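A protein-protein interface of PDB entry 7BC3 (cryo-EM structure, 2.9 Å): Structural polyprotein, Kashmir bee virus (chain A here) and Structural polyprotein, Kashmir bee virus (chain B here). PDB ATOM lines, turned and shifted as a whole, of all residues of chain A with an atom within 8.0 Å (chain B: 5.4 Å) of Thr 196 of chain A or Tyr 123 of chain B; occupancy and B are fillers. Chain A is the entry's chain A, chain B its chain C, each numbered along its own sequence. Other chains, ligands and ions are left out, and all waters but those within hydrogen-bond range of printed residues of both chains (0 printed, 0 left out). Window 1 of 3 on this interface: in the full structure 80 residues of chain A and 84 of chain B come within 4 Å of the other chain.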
ATOM      1  N   LEU A  39       0.678  14.227 -21.645  1.00  0.00           N
ATOM      2  CA  LEU A  39       1.700  15.250 -21.491  1.00  0.00           C
ATOM      3  C   LEU A  39       1.173  16.664 -21.694  1.00  0.00           C
ATOM      4  O   LEU A  39       1.942  17.620 -21.563  1.00  0.00           O
ATOM      5  CB  LEU A  39       2.852  14.976 -22.461  1.00  0.00           C
ATOM      6  CG  LEU A  39       3.531  13.625 -22.235  1.00  0.00           C
ATOM      7  CD1 LEU A  39       4.250  13.153 -23.482  1.00  0.00           C
ATOM      8  CD2 LEU A  39       4.490  13.703 -21.065  1.00  0.00           C
ATOM      9  N   GLU A  73      16.636  26.101 -25.177  1.00  0.00           N
ATOM     10  CA  GLU A  73      17.320  25.485 -24.044  1.00  0.00           C
ATOM     11  C   GLU A  73      16.780  24.088 -23.762  1.00  0.00           C
ATOM     12  O   GLU A  73      17.536  23.110 -23.741  1.00  0.00           O
ATOM     13  CB  GLU A  73      17.190  26.376 -22.810  1.00  0.00           C
ATOM     14  CG  GLU A  73      18.280  27.427 -22.710  1.00  0.00           C
ATOM     15  CD  GLU A  73      18.019  28.442 -21.618  1.00  0.00           C
ATOM     16  OE1 GLU A  73      16.955  28.360 -20.968  1.00  0.00           O
ATOM     17  OE2 GLU A  73      18.878  29.322 -21.408  1.00  0.00           O
ATOM     18  N   GLY A  74      15.471  23.973 -23.544  1.00  0.00           N
ATOM     19  CA  GLY A  74      14.869  22.702 -23.193  1.00  0.00           C
ATOM     20  C   GLY A  74      14.656  22.485 -21.715  1.00  0.00           C
ATOM     21  O   GLY A  74      14.529  21.333 -21.285  1.00  0.00           O
ATOM     22  N   ASP A  76      12.111  23.956 -19.680  1.00  0.00           N
ATOM     23  CA  ASP A  76      10.696  23.836 -19.374  1.00  0.00           C
ATOM     24  C   ASP A  76      10.054  22.750 -20.232  1.00  0.00           C
ATOM     25  O   ASP A  76      10.658  22.215 -21.165  1.00  0.00           O
ATOM     26  CB  ASP A  76       9.986  25.172 -19.585  1.00  0.00           C
ATOM     27  CG  ASP A  76      10.172  25.716 -20.984  1.00  0.00           C
ATOM     28  OD1 ASP A  76      11.290  25.592 -21.525  1.00  0.00           O
ATOM     29  OD2 ASP A  76       9.202  26.268 -21.543  1.00  0.00           O
ATOM     30  N   TYR A  77       8.804  22.427 -19.902  1.00  0.00           N
ATOM     31  CA  TYR A  77       8.098  21.374 -20.621  1.00  0.00           C
ATOM     32  C   TYR A  77       7.594  21.855 -21.973  1.00  0.00           C
ATOM     33  O   TYR A  77       7.502  21.062 -22.916  1.00  0.00           O
ATOM     34  CB  TYR A  77       6.938  20.856 -19.774  1.00  0.00           C
ATOM     35  CG  TYR A  77       7.364  20.206 -18.475  1.00  0.00           C
ATOM     36  CD1 TYR A  77       8.640  19.682 -18.321  1.00  0.00           C
ATOM     37  CD2 TYR A  77       6.490  20.116 -17.403  1.00  0.00           C
ATOM     38  CE1 TYR A  77       9.029  19.091 -17.141  1.00  0.00           C
ATOM     39  CE2 TYR A  77       6.871  19.524 -16.219  1.00  0.00           C
ATOM     40  CZ  TYR A  77       8.143  19.012 -16.093  1.00  0.00           C
ATOM     41  OH  TYR A  77       8.538  18.421 -14.918  1.00  0.00           O
ATOM     42  N   SER A  79       9.213  23.645 -23.922  1.00  0.00           N
ATOM     43  CA  SER A  79      10.379  23.584 -24.791  1.00  0.00           C
ATOM     44  C   SER A  79      10.850  22.150 -24.997  1.00  0.00           C
ATOM     45  O   SER A  79      11.046  21.713 -26.134  1.00  0.00           O
ATOM     46  CB  SER A  79      11.509  24.427 -24.198  1.00  0.00           C
ATOM     47  OG  SER A  79      12.609  24.501 -25.084  1.00  0.00           O
ATOM     48  N   TYR A  80      11.039  21.415 -23.900  1.00  0.00           N
ATOM     49  CA  TYR A  80      11.453  20.021 -23.987  1.00  0.00           C
ATOM     50  C   TYR A  80      10.555  19.238 -24.934  1.00  0.00           C
ATOM     51  O   TYR A  80      11.033  18.495 -25.797  1.00  0.00           O
ATOM     52  CB  TYR A  80      11.432  19.399 -22.592  1.00  0.00           C
ATOM     53  CG  TYR A  80      12.231  18.128 -22.454  1.00  0.00           C
ATOM     54  CD1 TYR A  80      13.616  18.147 -22.489  1.00  0.00           C
ATOM     55  CD2 TYR A  80      11.599  16.909 -22.277  1.00  0.00           C
ATOM     56  CE1 TYR A  80      14.346  16.986 -22.360  1.00  0.00           C
ATOM     57  CE2 TYR A  80      12.320  15.746 -22.148  1.00  0.00           C
ATOM     58  CZ  TYR A  80      13.691  15.789 -22.188  1.00  0.00           C
ATOM     59  OH  TYR A  80      14.407  14.624 -22.056  1.00  0.00           O
ATOM     60  N   LEU A  81       9.241  19.399 -24.786  1.00  0.00           N
ATOM     61  CA  LEU A  81       8.299  18.644 -25.602  1.00  0.00           C
ATOM     62  C   LEU A  81       8.221  19.171 -27.026  1.00  0.00           C
ATOM     63  O   LEU A  81       7.948  18.399 -27.950  1.00  0.00           O
ATOM     64  CB  LEU A  81       6.916  18.675 -24.956  1.00  0.00           C
ATOM     65  CG  LEU A  81       6.835  18.047 -23.565  1.00  0.00           C
ATOM     66  CD1 LEU A  81       5.453  18.233 -22.972  1.00  0.00           C
ATOM     67  CD2 LEU A  81       7.198  16.576 -23.618  1.00  0.00           C
ATOM     68  N   SER A  82       8.459  20.469 -27.228  1.00  0.00           N
ATOM     69  CA  SER A  82       8.424  21.020 -28.576  1.00  0.00           C
ATOM     70  C   SER A  82       9.412  20.313 -29.492  1.00  0.00           C
ATOM     71  O   SER A  82       9.177  20.212 -30.701  1.00  0.00           O
ATOM     72  CB  SER A  82       8.723  22.515 -28.536  1.00  0.00           C
ATOM     73  OG  SER A  82      10.070  22.750 -28.175  1.00  0.00           O
ATOM     74  N   PHE A  83      10.519  19.819 -28.938  1.00  0.00           N
ATOM     75  CA  PHE A  83      11.513  19.115 -29.733  1.00  0.00           C
ATOM     76  C   PHE A  83      11.020  17.763 -30.227  1.00  0.00           C
ATOM     77  O   PHE A  83      11.722  17.117 -31.012  1.00  0.00           O
ATOM     78  CB  PHE A  83      12.787  18.934 -28.914  1.00  0.00           C
ATOM     79  CG  PHE A  83      13.631  20.169 -28.832  1.00  0.00           C
ATOM     80  CD1 PHE A  83      14.540  20.470 -29.827  1.00  0.00           C
ATOM     81  CD2 PHE A  83      13.511  21.033 -27.760  1.00  0.00           C
ATOM     82  CE1 PHE A  83      15.315  21.605 -29.752  1.00  0.00           C
ATOM     83  CE2 PHE A  83      14.283  22.168 -27.681  1.00  0.00           C
ATOM     84  CZ  PHE A  83      15.187  22.456 -28.678  1.00  0.00           C
ATOM     85  N   LEU A  84       9.842  17.326 -29.789  1.00  0.00           N
ATOM     86  CA  LEU A  84       9.227  16.101 -30.275  1.00  0.00           C
ATOM     87  C   LEU A  84       8.202  16.350 -31.365  1.00  0.00           C
ATOM     88  O   LEU A  84       7.734  15.388 -31.984  1.00  0.00           O
ATOM     89  CB  LEU A  84       8.527  15.365 -29.131  1.00  0.00           C
ATOM     90  CG  LEU A  84       9.347  14.507 -28.181  1.00  0.00           C
ATOM     91  CD1 LEU A  84       8.409  13.890 -27.176  1.00  0.00           C
ATOM     92  CD2 LEU A  84      10.107  13.438 -28.926  1.00  0.00           C
ATOM     93  N   TYR A  85       7.836  17.604 -31.607  1.00  0.00           N
ATOM     94  CA  TYR A  85       6.736  17.928 -32.494  1.00  0.00           C
ATOM     95  C   TYR A  85       7.165  19.025 -33.454  1.00  0.00           C
ATOM     96  O   TYR A  85       8.253  19.593 -33.346  1.00  0.00           O
ATOM     97  CB  TYR A  85       5.495  18.360 -31.706  1.00  0.00           C
ATOM     98  CG  TYR A  85       5.035  17.354 -30.674  1.00  0.00           C
ATOM     99  CD1 TYR A  85       4.071  16.409 -30.980  1.00  0.00           C
ATOM    100  CD2 TYR A  85       5.554  17.360 -29.392  1.00  0.00           C
ATOM    101  CE1 TYR A  85       3.648  15.496 -30.052  1.00  0.00           C
ATOM    102  CE2 TYR A  85       5.134  16.447 -28.452  1.00  0.00           C
ATOM    103  CZ  TYR A  85       4.182  15.516 -28.790  1.00  0.00           C
ATOM    104  OH  TYR A  85       3.753  14.601 -27.861  1.00  0.00           O
ATOM    105  N   MET A 193       4.105  13.884 -34.169  1.00  0.00           N
ATOM    106  CA  MET A 193       5.146  13.298 -33.350  1.00  0.00           C
ATOM    107  C   MET A 193       6.303  12.883 -34.247  1.00  0.00           C
ATOM    108  O   MET A 193       6.114  12.140 -35.216  1.00  0.00           O
ATOM    109  CB  MET A 193       4.604  12.105 -32.577  1.00  0.00           C
ATOM    110  CG  MET A 193       5.331  11.837 -31.284  1.00  0.00           C
ATOM    111  SD  MET A 193       4.628  10.424 -30.432  1.00  0.00           S
ATOM    112  CE  MET A 193       4.942   9.150 -31.643  1.00  0.00           C
ATOM    113  N   ILE A 194       7.498  13.370 -33.927  1.00  0.00           N
ATOM    114  CA  ILE A 194       8.701  13.094 -34.688  1.00  0.00           C
ATOM    115  C   ILE A 194       9.740  12.510 -33.740  1.00  0.00           C
ATOM    116  O   ILE A 194       9.479  12.286 -32.560  1.00  0.00           O
ATOM    117  CB  ILE A 194       9.255  14.350 -35.394  1.00  0.00           C
ATOM    118  CG1 ILE A 194       9.388  15.501 -34.401  1.00  0.00           C
ATOM    119  CG2 ILE A 194       8.375  14.749 -36.563  1.00  0.00           C
ATOM    120  CD1 ILE A 194      10.467  16.471 -34.756  1.00  0.00           C
ATOM    121  N   GLY A 195      10.925  12.264 -34.276  1.00  0.00           N
ATOM    122  CA  GLY A 195      11.993  11.704 -33.485  1.00  0.00           C
ATOM    123  C   GLY A 195      12.553  12.690 -32.483  1.00  0.00           C
ATOM    124  O   GLY A 195      12.242  13.882 -32.474  1.00  0.00           O
ATOM    125  N   THR A 196      13.397  12.165 -31.622  1.00  0.00           N
ATOM    126  CA  THR A 196      13.990  12.912 -30.530  1.00  0.00           C
ATOM    127  C   THR A 196      15.306  13.543 -30.957  1.00  0.00           C
ATOM    128  O   THR A 196      15.973  13.060 -31.876  1.00  0.00           O
ATOM    129  CB  THR A 196      14.236  11.987 -29.343  1.00  0.00           C
ATOM    130  OG1 THR A 196      15.202  10.995 -29.704  1.00  0.00           O
ATOM    131  CG2 THR A 196      12.961  11.301 -28.931  1.00  0.00           C
ATOM    132  N   PRO A 197      15.709  14.635 -30.308  1.00  0.00           N
ATOM    133  CA  PRO A 197      17.084  15.113 -30.467  1.00  0.00           C
ATOM    134  C   PRO A 197      18.002  14.501 -29.425  1.00  0.00           C
ATOM    135  O   PRO A 197      17.554  13.728 -28.574  1.00  0.00           O
ATOM    136  CB  PRO A 197      16.945  16.625 -30.286  1.00  0.00           C
ATOM    137  CG  PRO A 197      15.821  16.769 -29.334  1.00  0.00           C
ATOM    138  CD  PRO A 197      14.905  15.576 -29.510  1.00  0.00           C
ATOM    139  N   GLN A 198      19.284  14.837 -29.480  1.00  0.00           N
ATOM    140  CA  GLN A 198      20.227  14.353 -28.487  1.00  0.00           C
ATOM    141  C   GLN A 198      20.172  15.226 -27.241  1.00  0.00           C
ATOM    142  O   GLN A 198      19.899  16.428 -27.309  1.00  0.00           O
ATOM    143  CB  GLN A 198      21.640  14.337 -29.062  1.00  0.00           C
ATOM    144  CG  GLN A 198      21.820  13.343 -30.195  1.00  0.00           C
ATOM    145  CD  GLN A 198      23.098  13.562 -30.970  1.00  0.00           C
ATOM    146  OE1 GLN A 198      23.909  12.650 -31.122  1.00  0.00           O
ATOM    147  NE2 GLN A 198      23.284  14.774 -31.473  1.00  0.00           N
ATOM    148  N   LEU A 199      20.428  14.608 -26.093  1.00  0.00           N
ATOM    149  CA  LEU A 199      20.331  15.278 -24.807  1.00  0.00           C
ATOM    150  C   LEU A 199      21.717  15.578 -24.251  1.00  0.00           C
ATOM    151  O   LEU A 199      22.671  14.825 -24.461  1.00  0.00           O
ATOM    152  CB  LEU A 199      19.549  14.431 -23.801  1.00  0.00           C
ATOM    153  CG  LEU A 199      18.083  14.187 -24.148  1.00  0.00           C
ATOM    154  CD1 LEU A 199      17.469  13.160 -23.215  1.00  0.00           C
ATOM    155  CD2 LEU A 199      17.304  15.486 -24.096  1.00  0.00           C
ATOM    156  N   PRO B 118      18.663   9.205 -27.176  1.00  0.00           N
ATOM    157  CA  PRO B 118      17.453   8.639 -26.578  1.00  0.00           C
ATOM    158  C   PRO B 118      16.361   8.313 -27.580  1.00  0.00           C
ATOM    159  O   PRO B 118      16.149   9.012 -28.573  1.00  0.00           O
ATOM    160  CB  PRO B 118      16.996   9.751 -25.625  1.00  0.00           C
ATOM    161  CG  PRO B 118      17.593  11.020 -26.169  1.00  0.00           C
ATOM    162  CD  PRO B 118      18.583  10.671 -27.252  1.00  0.00           C
ATOM    163  N   ALA B 119      15.663   7.221 -27.299  1.00  0.00           N
ATOM    164  CA  ALA B 119      14.404   6.924 -27.950  1.00  0.00           C
ATOM    165  C   ALA B 119      13.296   7.698 -27.252  1.00  0.00           C
ATOM    166  O   ALA B 119      13.489   8.239 -26.162  1.00  0.00           O
ATOM    167  CB  ALA B 119      14.145   5.421 -27.914  1.00  0.00           C
ATOM    168  N   PRO B 120      12.114   7.782 -27.861  1.00  0.00           N
ATOM    169  CA  PRO B 120      11.031   8.548 -27.226  1.00  0.00           C
ATOM    170  C   PRO B 120      10.737   8.110 -25.801  1.00  0.00           C
ATOM    171  O   PRO B 120      10.445   8.955 -24.945  1.00  0.00           O
ATOM    172  CB  PRO B 120       9.845   8.300 -28.166  1.00  0.00           C
ATOM    173  CG  PRO B 120      10.470   8.005 -29.481  1.00  0.00           C
ATOM    174  CD  PRO B 120      11.714   7.248 -29.173  1.00  0.00           C
ATOM    175  N   CYS B 121      10.815   6.809 -25.520  1.00  0.00           N
ATOM    176  CA  CYS B 121      10.640   6.344 -24.149  1.00  0.00           C
ATOM    177  C   CYS B 121      11.684   6.958 -23.224  1.00  0.00           C
ATOM    178  O   CYS B 121      11.366   7.372 -22.105  1.00  0.00           O
ATOM    179  CB  CYS B 121      10.708   4.818 -24.105  1.00  0.00           C
ATOM    180  SG  CYS B 121      12.219   4.116 -24.788  1.00  0.00           S
ATOM    181  N   GLU B 122      12.934   7.046 -23.684  1.00  0.00           N
ATOM    182  CA  GLU B 122      13.988   7.623 -22.856  1.00  0.00           C
ATOM    183  C   GLU B 122      13.807   9.129 -22.713  1.00  0.00           C
ATOM    184  O   GLU B 122      13.999   9.687 -21.624  1.00  0.00           O
ATOM    185  CB  GLU B 122      15.356   7.290 -23.457  1.00  0.00           C
ATOM    186  CG  GLU B 122      15.638   5.794 -23.561  1.00  0.00           C
ATOM    187  CD  GLU B 122      16.971   5.467 -24.190  1.00  0.00           C
ATOM    188  OE1 GLU B 122      17.753   6.397 -24.455  1.00  0.00           O
ATOM    189  OE2 GLU B 122      17.237   4.269 -24.424  1.00  0.00           O
ATOM    190  N   TYR B 123      13.442   9.801 -23.806  1.00  0.00           N
ATOM    191  CA  TYR B 123      13.124  11.222 -23.748  1.00  0.00           C
ATOM    192  C   TYR B 123      12.055  11.504 -22.702  1.00  0.00           C
ATOM    193  O   TYR B 123      12.161  12.465 -21.933  1.00  0.00           O
ATOM    194  CB  TYR B 123      12.663  11.692 -25.128  1.00  0.00           C
ATOM    195  CG  TYR B 123      12.795  13.174 -25.380  1.00  0.00           C
ATOM    196  CD1 TYR B 123      14.031  13.751 -25.620  1.00  0.00           C
ATOM    197  CD2 TYR B 123      11.677  13.994 -25.398  1.00  0.00           C
ATOM    198  CE1 TYR B 123      14.152  15.103 -25.859  1.00  0.00           C
ATOM    199  CE2 TYR B 123      11.789  15.345 -25.635  1.00  0.00           C
ATOM    200  CZ  TYR B 123      13.026  15.895 -25.865  1.00  0.00           C
ATOM    201  OH  TYR B 123      13.136  17.244 -26.102  1.00  0.00           O
ATOM    202  N   VAL B 124      11.016  10.670 -22.660  1.00  0.00           N
ATOM    203  CA  VAL B 124       9.941  10.865 -21.693  1.00  0.00           C
ATOM    204  C   VAL B 124      10.431  10.569 -20.282  1.00  0.00           C
ATOM    205  O   VAL B 124      10.181  11.337 -19.346  1.00  0.00           O
ATOM    206  CB  VAL B 124       8.730   9.989 -22.060  1.00  0.00           C
ATOM    207  CG1 VAL B 124       7.706   9.995 -20.940  1.00  0.00           C
ATOM    208  CG2 VAL B 124       8.111  10.460 -23.364  1.00  0.00           C
ATOM    209  N   ALA B 125      11.130   9.447 -20.103  1.00  0.00           N
ATOM    210  CA  ALA B 125      11.573   9.057 -18.769  1.00  0.00           C
ATOM    211  C   ALA B 125      12.475  10.116 -18.151  1.00  0.00           C
ATOM    212  O   ALA B 125      12.416  10.360 -16.941  1.00  0.00           O
ATOM    213  CB  ALA B 125      12.291   7.711 -18.831  1.00  0.00           C
ATOM    214  N   ASN B 126      13.316  10.761 -18.964  1.00  0.00           N
ATOM    215  CA  ASN B 126      14.202  11.794 -18.436  1.00  0.00           C
ATOM    216  C   ASN B 126      13.444  12.912 -17.731  1.00  0.00           C
ATOM    217  O   ASN B 126      14.045  13.650 -16.945  1.00  0.00           O
ATOM    218  CB  ASN B 126      15.051  12.384 -19.561  1.00  0.00           C
ATOM    219  CG  ASN B 126      16.130  13.309 -19.051  1.00  0.00           C
ATOM    220  OD1 ASN B 126      15.846  14.374 -18.502  1.00  0.00           O
ATOM    221  ND2 ASN B 126      17.380  12.906 -19.223  1.00  0.00           N
ATOM    222  N   LEU B 127      12.144  13.046 -17.980  1.00  0.00           N
ATOM    223  CA  LEU B 127      11.360  14.117 -17.381  1.00  0.00           C
ATOM    224  C   LEU B 127      10.877  13.794 -15.978  1.00  0.00           C
ATOM    225  O   LEU B 127      10.292  14.667 -15.329  1.00  0.00           O
ATOM    226  CB  LEU B 127      10.143  14.426 -18.250  1.00  0.00           C
ATOM    227  CG  LEU B 127      10.285  15.517 -19.302  1.00  0.00           C
ATOM    228  CD1 LEU B 127       8.955  15.728 -19.988  1.00  0.00           C
ATOM    229  CD2 LEU B 127      10.787  16.805 -18.686  1.00  0.00           C
ATOM    230  N   VAL B 280      18.767  20.124 -24.043  1.00  0.00           N
ATOM    231  CA  VAL B 280      18.872  19.515 -25.361  1.00  0.00           C
ATOM    232  C   VAL B 280      20.223  19.880 -25.955  1.00  0.00           C
ATOM    233  O   VAL B 280      20.630  21.047 -25.931  1.00  0.00           O
ATOM    234  CB  VAL B 280      17.726  19.976 -26.275  1.00  0.00           C
ATOM    235  CG1 VAL B 280      17.902  19.404 -27.667  1.00  0.00           C
ATOM    236  CG2 VAL B 280      16.383  19.567 -25.693  1.00  0.00           C
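Among the printed residues, merely in contact across the chains: Tyr 77 of chain A with Leu 127 of chain B, Phe 83 of chain A with Tyr 123 of chain B, Tyr 80 of chain A with Asn 126 of chain B, Pro 197 of chain A with Pro 118 of chain B, Tyr 80 of chain A with Leu 127 of chain B, Gln 198 of chain A with Val 280 of chain B, Leu 84 of chain A with Tyr 123 of chain B, Leu 199 of chain A with Tyr 123 of chain B, Leu 199 of chain A with Pro 118 of chain B, Pro 197 of chain A with Val 280 of chain B, Pro 197 of chain A with Tyr 123 of chain B, Thr 196 of chain A with Pro 120 of chain B, Phe 83 of chain A with Val 280 of chain B, Thr 196 of chain A with Tyr 123 of chain B and Thr 196 of chain A with Ala 119 of chain B.
Of the printed residues of chain B, Thr 196 of chain A touches Pro 118, Ala 119, Pro 120 and Tyr 123. Tyr 123 of chain B touches just these residues of chain A: Tyr 80 (2.5 Å), Phe 83 (3.3 Å), Leu 84 (3.6 Å), Thr 196 (3.8 Å), Pro 197 (3.8 Å) and Leu 199 (3.6 Å). Of the printed residues of chain A, Val 280 of chain B touches Glu 73, Phe 83, Pro 197 and Gln 198. Printed residues of chain B within 4 Å of Tyr 80 of chain A: Tyr 123, Asn 126 and Leu 127. The nearest printed residue of chain B that does not touch Phe 83 of chain A is Pro 120 of chain B (9.3 Å).
The backbone carbonyl oxygen (O) of Leu 84 of chain A sits at hydrogen-bond distance from the backbone NH (N) of Ile 194 of chain A.
Of the 19 printed residues of chain A, 9 touch a printed residue of chain B. Printed residues of chain A that touch a printed residue of chain B: Glu 73, Tyr 77, Tyr 80, Phe 83, Leu 84, Thr 196, Pro 197, Gln 198 and Leu 199. Hydrophobic or aromatic side chains of chain A that line the printed part of chain B: Tyr 77, Tyr 80, Phe 83, Leu 84, Pro 197 and Leu 199. Along chain A the printed residues that touch a printed residue of chain B span positions 73 to 199. Of the 11 printed residues of chain B, 7 touch a printed residue of chain A. Hydrophobic or aromatic side chains of chain B within 4 Å of the printed part of chain A: Pro 118, Tyr 123, Leu 127 and Val 280.
N of Val 280 of chain B lies within hydrogen-bond range of O of Glu 73 of chain A (3.2 Å). The backbone carbonyl oxygen (O) of Tyr 80 of chain A lies within hydrogen-bond range of the side-chain hydroxyl (OH) of Tyr 123 of chain B (2.5 Å). The backbone carbonyl oxygen (O) of Pro 118 of chain B is in hydrogen-bond range of the side-chain hydroxyl (OG1) of Thr 196 of chain A, at 2.5 Å.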
